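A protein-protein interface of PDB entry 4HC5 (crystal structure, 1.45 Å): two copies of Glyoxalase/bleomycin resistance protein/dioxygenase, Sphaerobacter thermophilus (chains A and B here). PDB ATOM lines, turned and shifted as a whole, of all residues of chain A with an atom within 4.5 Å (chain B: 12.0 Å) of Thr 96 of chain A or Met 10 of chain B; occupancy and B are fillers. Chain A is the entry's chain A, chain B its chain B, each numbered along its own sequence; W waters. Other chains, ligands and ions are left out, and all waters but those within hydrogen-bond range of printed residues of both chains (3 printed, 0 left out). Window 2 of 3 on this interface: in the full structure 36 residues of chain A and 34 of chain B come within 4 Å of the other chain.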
ATOM      1  N   LEU A  35      -9.787   4.544 -27.362  1.00  0.00           N
ATOM      2  CA  LEU A  35     -11.124   4.053 -27.016  1.00  0.00           C
ATOM      3  C   LEU A  35     -12.234   4.519 -27.922  1.00  0.00           C
ATOM      4  O   LEU A  35     -13.350   4.024 -27.856  1.00  0.00           O
ATOM      5  CB  LEU A  35     -11.507   4.277 -25.566  1.00  0.00           C
ATOM      6  CG  LEU A  35     -10.609   3.658 -24.486  1.00  0.00           C
ATOM      7  CD1 LEU A  35     -11.212   3.878 -23.101  1.00  0.00           C
ATOM      8  CD2 LEU A  35     -10.302   2.188 -24.764  1.00  0.00           C
ATOM      9  N   THR A  87     -20.286  -2.394 -24.337  1.00  0.00           N
ATOM     10  CA  THR A  87     -19.982  -2.524 -25.750  1.00  0.00           C
ATOM     11  C   THR A  87     -21.022  -3.488 -26.337  1.00  0.00           C
ATOM     12  O   THR A  87     -21.499  -4.379 -25.661  1.00  0.00           O
ATOM     13  CB  THR A  87     -18.544  -3.065 -25.995  1.00  0.00           C
ATOM     14  OG1 THR A  87     -18.296  -3.105 -27.396  1.00  0.00           O
ATOM     15  CG2 THR A  87     -18.348  -4.463 -25.393  1.00  0.00           C
ATOM     16  N   GLU A  92     -14.945  -8.129 -30.607  1.00  0.00           N
ATOM     17  CA  GLU A  92     -14.314  -7.118 -31.453  1.00  0.00           C
ATOM     18  C   GLU A  92     -13.587  -6.079 -30.626  1.00  0.00           C
ATOM     19  O   GLU A  92     -12.486  -5.654 -30.970  1.00  0.00           O
ATOM     20  CB  GLU A  92     -15.338  -6.458 -32.358  1.00  0.00           C
ATOM     21  CG  GLU A  92     -14.697  -5.537 -33.361  1.00  0.00           C
ATOM     22  CD  GLU A  92     -13.818  -6.307 -34.379  1.00  0.00           C
ATOM     23  OE1 GLU A  92     -12.879  -5.692 -34.891  1.00  0.00           O
ATOM     24  OE2 GLU A  92     -14.035  -7.531 -34.663  1.00  0.00           O
ATOM     25  N   ALA A  93     -14.224  -5.640 -29.532  1.00  0.00           N
ATOM     26  CA  ALA A  93     -13.593  -4.627 -28.656  1.00  0.00           C
ATOM     27  C   ALA A  93     -12.266  -5.182 -28.103  1.00  0.00           C
ATOM     28  O   ALA A  93     -11.219  -4.514 -28.106  1.00  0.00           O
ATOM     29  CB  ALA A  93     -14.505  -4.148 -27.525  1.00  0.00           C
ATOM     30  N   TYR A  94     -12.336  -6.388 -27.608  1.00  0.00           N
ATOM     31  CA  TYR A  94     -11.136  -7.014 -27.069  1.00  0.00           C
ATOM     32  C   TYR A  94     -10.017  -7.135 -28.129  1.00  0.00           C
ATOM     33  O   TYR A  94      -8.855  -6.806 -27.863  1.00  0.00           O
ATOM     34  CB  TYR A  94     -11.439  -8.381 -26.469  1.00  0.00           C
ATOM     35  CG  TYR A  94     -10.257  -9.189 -26.024  1.00  0.00           C
ATOM     36  CD1 TYR A  94      -9.599  -8.931 -24.849  1.00  0.00           C
ATOM     37  CD2 TYR A  94      -9.765 -10.193 -26.805  1.00  0.00           C
ATOM     38  CE1 TYR A  94      -8.483  -9.650 -24.456  1.00  0.00           C
ATOM     39  CE2 TYR A  94      -8.630 -10.915 -26.439  1.00  0.00           C
ATOM     40  CZ  TYR A  94      -7.989 -10.645 -25.268  1.00  0.00           C
ATOM     41  OH  TYR A  94      -6.873 -11.407 -24.879  1.00  0.00           O
ATOM     42  N   LYS A  95     -10.354  -7.616 -29.323  1.00  0.00           N
ATOM     43  CA  LYS A  95      -9.402  -7.821 -30.392  1.00  0.00           C
ATOM     44  C   LYS A  95      -8.784  -6.462 -30.766  1.00  0.00           C
ATOM     45  O   LYS A  95      -7.542  -6.319 -30.809  1.00  0.00           O
ATOM     46  CB  LYS A  95     -10.068  -8.456 -31.588  1.00  0.00           C
ATOM     47  CG  LYS A  95      -9.064  -8.805 -32.685  1.00  0.00           C
ATOM     48  CD  LYS A  95      -9.786  -9.687 -33.668  1.00  0.00           C
ATOM     49  CE  LYS A  95      -9.896  -9.095 -35.037  1.00  0.00           C
ATOM     50  NZ  LYS A  95      -8.684  -9.483 -35.776  1.00  0.00           N
ATOM     51  N   THR A  96      -9.645  -5.485 -31.119  1.00  0.00           N
ATOM     52  CA  THR A  96      -9.109  -4.237 -31.659  1.00  0.00           C
ATOM     53  C   THR A  96      -8.409  -3.422 -30.569  1.00  0.00           C
ATOM     54  O   THR A  96      -7.348  -2.884 -30.762  1.00  0.00           O
ATOM     55  CB  THR A  96     -10.211  -3.447 -32.292  1.00  0.00           C
ATOM     56  OG1 THR A  96     -10.754  -4.280 -33.357  1.00  0.00           O
ATOM     57  CG2 THR A  96      -9.772  -2.065 -32.769  1.00  0.00           C
ATOM     58  N   LEU A  97      -8.996  -3.369 -29.379  1.00  0.00           N
ATOM     59  CA  LEU A  97      -8.309  -2.640 -28.295  1.00  0.00           C
ATOM     60  C   LEU A  97      -6.961  -3.261 -27.904  1.00  0.00           C
ATOM     61  O   LEU A  97      -6.003  -2.563 -27.626  1.00  0.00           O
ATOM     62  CB  LEU A  97      -9.187  -2.444 -27.048  1.00  0.00           C
ATOM     63  CG  LEU A  97     -10.429  -1.522 -27.263  1.00  0.00           C
ATOM     64  CD1 LEU A  97     -11.249  -1.453 -25.958  1.00  0.00           C
ATOM     65  CD2 LEU A  97     -10.059  -0.119 -27.779  1.00  0.00           C
ATOM     66  N   THR A  98      -6.892  -4.609 -27.916  1.00  0.00           N
ATOM     67  CA  THR A  98      -5.595  -5.274 -27.675  1.00  0.00           C
ATOM     68  C   THR A  98      -4.564  -4.871 -28.763  1.00  0.00           C
ATOM     69  O   THR A  98      -3.429  -4.586 -28.461  1.00  0.00           O
ATOM     70  CB  THR A  98      -5.750  -6.801 -27.652  1.00  0.00           C
ATOM     71  OG1 THR A  98      -6.520  -7.127 -26.493  1.00  0.00           O
ATOM     72  CG2 THR A  98      -4.416  -7.526 -27.517  1.00  0.00           C
ATOM     73  N   GLU A  99      -4.982  -4.884 -30.018  1.00  0.00           N
ATOM     74  CA  GLU A  99      -4.129  -4.435 -31.171  1.00  0.00           C
ATOM     75  C   GLU A  99      -3.584  -2.993 -30.975  1.00  0.00           C
ATOM     76  O   GLU A  99      -2.477  -2.677 -31.289  1.00  0.00           O
ATOM     77  CB  GLU A  99      -4.883  -4.519 -32.488  1.00  0.00           C
ATOM     78  CG  GLU A  99      -5.159  -5.904 -33.028  1.00  0.00           C
ATOM     79  CD  GLU A  99      -6.076  -5.901 -34.259  1.00  0.00           C
ATOM     80  OE1 GLU A  99      -6.372  -4.802 -34.807  1.00  0.00           O
ATOM     81  OE2 GLU A  99      -6.502  -7.021 -34.657  1.00  0.00           O
ATOM     82  N   ARG A 100      -4.410  -2.170 -30.300  1.00  0.00           N
ATOM     83  CA  ARG A 100      -4.162  -0.753 -30.074  1.00  0.00           C
ATOM     84  C   ARG A 100      -3.330  -0.514 -28.813  1.00  0.00           C
ATOM     85  O   ARG A 100      -3.007   0.614 -28.466  1.00  0.00           O
ATOM     86  CB  ARG A 100      -5.433   0.071 -30.020  1.00  0.00           C
ATOM     87  CG  ARG A 100      -6.155   0.188 -31.327  1.00  0.00           C
ATOM     88  CD  ARG A 100      -7.418   1.000 -31.221  1.00  0.00           C
ATOM     89  NE  ARG A 100      -8.185   1.017 -32.438  1.00  0.00           N
ATOM     90  CZ  ARG A 100      -9.364   1.550 -32.569  1.00  0.00           C
ATOM     91  NH1 ARG A 100      -9.954   1.491 -33.740  1.00  0.00           N
ATOM     92  NH2 ARG A 100      -9.924   2.168 -31.540  1.00  0.00           N
ATOM     93  N   SER B   8     -18.811  -2.005 -35.193  1.00  0.00           N
ATOM     94  CA  SER B   8     -19.385  -1.682 -33.841  1.00  0.00           C
ATOM     95  C   SER B   8     -18.475  -0.650 -33.140  1.00  0.00           C
ATOM     96  O   SER B   8     -17.291  -0.643 -33.360  1.00  0.00           O
ATOM     97  CB  SER B   8     -19.482  -2.931 -32.963  1.00  0.00           C
ATOM     98  OG  SER B   8     -18.221  -3.627 -32.948  1.00  0.00           O
ATOM     99  N   LEU B   9     -19.043   0.202 -32.295  1.00  0.00           N
ATOM    100  CA  LEU B   9     -18.207   1.058 -31.384  1.00  0.00           C
ATOM    101  C   LEU B   9     -17.386   0.223 -30.432  1.00  0.00           C
ATOM    102  O   LEU B   9     -17.837  -0.861 -29.975  1.00  0.00           O
ATOM    103  CB  LEU B   9     -19.085   2.001 -30.549  1.00  0.00           C
ATOM    104  CG  LEU B   9     -19.940   3.074 -31.269  1.00  0.00           C
ATOM    105  CD1 LEU B   9     -20.906   3.858 -30.301  1.00  0.00           C
ATOM    106  CD2 LEU B   9     -19.022   4.006 -32.089  1.00  0.00           C
ATOM    107  N   MET B  10     -16.167   0.672 -30.149  1.00  0.00           N
ATOM    108  CA  MET B  10     -15.389   0.001 -29.076  1.00  0.00           C
ATOM    109  C   MET B  10     -16.253   0.028 -27.799  1.00  0.00           C
ATOM    110  O   MET B  10     -16.398  -0.970 -27.119  1.00  0.00           O
ATOM    111  CB  MET B  10     -14.032   0.663 -28.829  1.00  0.00           C
ATOM    112  CG  MET B  10     -13.117   0.601 -30.032  1.00  0.00           C
ATOM    113  SD  MET B  10     -12.578  -1.137 -30.476  1.00  0.00           S
ATOM    114  CE  MET B  10     -13.891  -1.679 -31.768  1.00  0.00           C
ATOM    115  N   ILE B  11     -16.731   1.237 -27.476  1.00  0.00           N
ATOM    116  CA  ILE B  11     -17.504   1.529 -26.250  1.00  0.00           C
ATOM    117  C   ILE B  11     -18.749   2.305 -26.648  1.00  0.00           C
ATOM    118  O   ILE B  11     -18.645   3.383 -27.241  1.00  0.00           O
ATOM    119  CB  ILE B  11     -16.704   2.395 -25.201  1.00  0.00           C
ATOM    120  CG1 ILE B  11     -15.296   1.772 -24.900  1.00  0.00           C
ATOM    121  CG2 ILE B  11     -17.536   2.715 -23.943  1.00  0.00           C
ATOM    122  CD1 ILE B  11     -15.308   0.432 -24.271  1.00  0.00           C
ATOM    123  N   ALA B  12     -19.929   1.781 -26.239  1.00  0.00           N
ATOM    124  CA  ALA B  12     -21.236   2.338 -26.598  1.00  0.00           C
ATOM    125  C   ALA B  12     -21.744   3.399 -25.623  1.00  0.00           C
ATOM    126  O   ALA B  12     -22.280   4.406 -26.023  1.00  0.00           O
ATOM    127  CB  ALA B  12     -22.264   1.225 -26.751  1.00  0.00           C
ATOM    128  N   TYR B  13     -21.575   3.148 -24.331  1.00  0.00           N
ATOM    129  CA  TYR B  13     -22.020   4.069 -23.279  1.00  0.00           C
ATOM    130  C   TYR B  13     -21.511   3.620 -21.918  1.00  0.00           C
ATOM    131  O   TYR B  13     -21.070   2.487 -21.709  1.00  0.00           O
ATOM    132  CB  TYR B  13     -23.560   4.227 -23.217  1.00  0.00           C
ATOM    133  CG  TYR B  13     -24.353   2.986 -22.937  1.00  0.00           C
ATOM    134  CD1 TYR B  13     -24.716   2.150 -24.016  1.00  0.00           C
ATOM    135  CD2 TYR B  13     -24.804   2.658 -21.672  1.00  0.00           C
ATOM    136  CE1 TYR B  13     -25.554   1.059 -23.821  1.00  0.00           C
ATOM    137  CE2 TYR B  13     -25.594   1.525 -21.445  1.00  0.00           C
ATOM    138  CZ  TYR B  13     -25.929   0.728 -22.530  1.00  0.00           C
ATOM    139  OH  TYR B  13     -26.708  -0.383 -22.360  1.00  0.00           O
ATOM    140  N   VAL B  14     -21.554   4.593 -21.028  1.00  0.00           N
ATOM    141  CA  VAL B  14     -21.264   4.337 -19.616  1.00  0.00           C
ATOM    142  C   VAL B  14     -22.460   3.692 -18.914  1.00  0.00           C
ATOM    143  O   VAL B  14     -23.585   4.278 -18.880  1.00  0.00           O
ATOM    144  CB  VAL B  14     -20.883   5.634 -18.836  1.00  0.00           C
ATOM    145  CG1 VAL B  14     -20.642   5.318 -17.359  1.00  0.00           C
ATOM    146  CG2 VAL B  14     -19.689   6.352 -19.529  1.00  0.00           C
ATOM    147  N   HIS B  15     -22.284   2.489 -18.381  1.00  0.00           N
ATOM    148  CA  HIS B  15     -23.396   1.785 -17.761  1.00  0.00           C
ATOM    149  C   HIS B  15     -23.774   2.396 -16.451  1.00  0.00           C
ATOM    150  O   HIS B  15     -24.969   2.601 -16.146  1.00  0.00           O
ATOM    151  CB  HIS B  15     -23.046   0.323 -17.534  1.00  0.00           C
ATOM    152  CG  HIS B  15     -24.118  -0.455 -16.807  1.00  0.00           C
ATOM    153  ND1 HIS B  15     -24.150  -0.564 -15.468  1.00  0.00           N
ATOM    154  CD2 HIS B  15     -25.213  -1.170 -17.287  1.00  0.00           C
ATOM    155  CE1 HIS B  15     -25.210  -1.310 -15.104  1.00  0.00           C
ATOM    156  NE2 HIS B  15     -25.860  -1.680 -16.219  1.00  0.00           N
HETATM  157  O   HOH W   1     -16.048   3.875 -28.666  1.00  0.00           O
HETATM  158  O   HOH W   2     -17.021  -3.511 -30.474  1.00  0.00           O
HETATM  159  O   HOH W   3     -20.476  -1.042 -29.126  1.00  0.00           O
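O of Met 10 of chain B lies within hydrogen-bond range of OG1 of Thr 87 of chain A (2.9 Å). The side-chain hydroxyl (OG1) of Thr 87 of chain A is in hydrogen-bond range of the backbone carbonyl oxygen (O) of Leu 9 of chain B, 3.4 Å away.
The side-chain carboxylate of Glu 92 of chain A is in hydrogen-bond range of the side-chain hydroxyl of Thr 96 of chain A (3.0 Å).
Leu 35 of chain A touches Met 10 of chain B. Met 10 of chain B touches Ala 93 of chain A (O to CB, 3.7 Å). Met 10 of chain B touches Thr 96 of chain A. Leu 97 of chain A touches Met 10 of chain B. NH2 of Arg 100 of chain A touches CG of Met 10 of chain B, 3.9 Å away.
Leu 35 of chain A touches just one residue of chain B: Met 10. Of chain B, only Leu 9 and Met 10 come within 4 Å of Thr 87 of chain A. No residue of chain B comes within 4 Å of Glu 92 of chain A. Printed residues of chain B within 4 Å of Ala 93 of chain A: Met 10. No residue of chain B comes within 4 Å of Lys 95 of chain A. Of chain B, only Met 10 (3.7 Å) comes within 4 Å of Thr 96 of chain A. Printed residues of chain B within 4 Å of Leu 97 of chain A: Met 10 (3.8 Å). No residue of chain B comes within 4 Å of Thr 98 of chain A. Arg 100 of chain A touches just one residue of chain B: Met 10 (3.9 Å). Of the printed residues of chain A, Leu 9 of chain B touches Thr 87 (3.4 Å). Ala 12 of chain B touches none of the printed residues of chain A. His 15 of chain B touches none of the printed residues of chain A. The nearest residue of chain B that does not touch Thr 96 of chain A is Ser 8 of chain B (7.5 Å). The nearest residue of chain A that does not touch Met 10 of chain B is Glu 92 of chain A (4.3 Å). The nearest printed residue of chain A that does not touch Leu 9 of chain B is Ala 93 of chain A (5.3 Å).
Printed residues of chain B that touch a printed residue of chain A: Leu 9 and Met 10. Hydrophobic or aromatic side chains of chain B within 4 Å of the printed part of chain A: Met 10. Printed residues of chain A that touch a printed residue of chain B: Leu 35, Thr 87, Ala 93, Thr 96, Leu 97 and Arg 100. Hydrophobic or aromatic side chains of chain A that line the printed part of chain B: Ala 93 and Leu 97. Among the printed residues, no Asp or Glu carboxylate lies within 4 Å of a Lys or Arg side-chain nitrogen of the other chain.
No position is printed for both chains.
Water W2 lies within hydrogen-bond range of OG of Ser 8 of chain B (2.8 Å), O of Leu 9 of chain B (2.8 Å) and OG1 of Thr 87 of chain A (3.4 Å). Water W3 bridges the backbone carbonyl oxygen of Leu 9 of chain B (2.8 Å) and the side-chain hydroxyl of Thr 87 of chain A (3.5 Å). Water W1 bridges O of Leu 35 of chain A (2.8 Å) and N of Ile 11 of chain B (3.0 Å).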
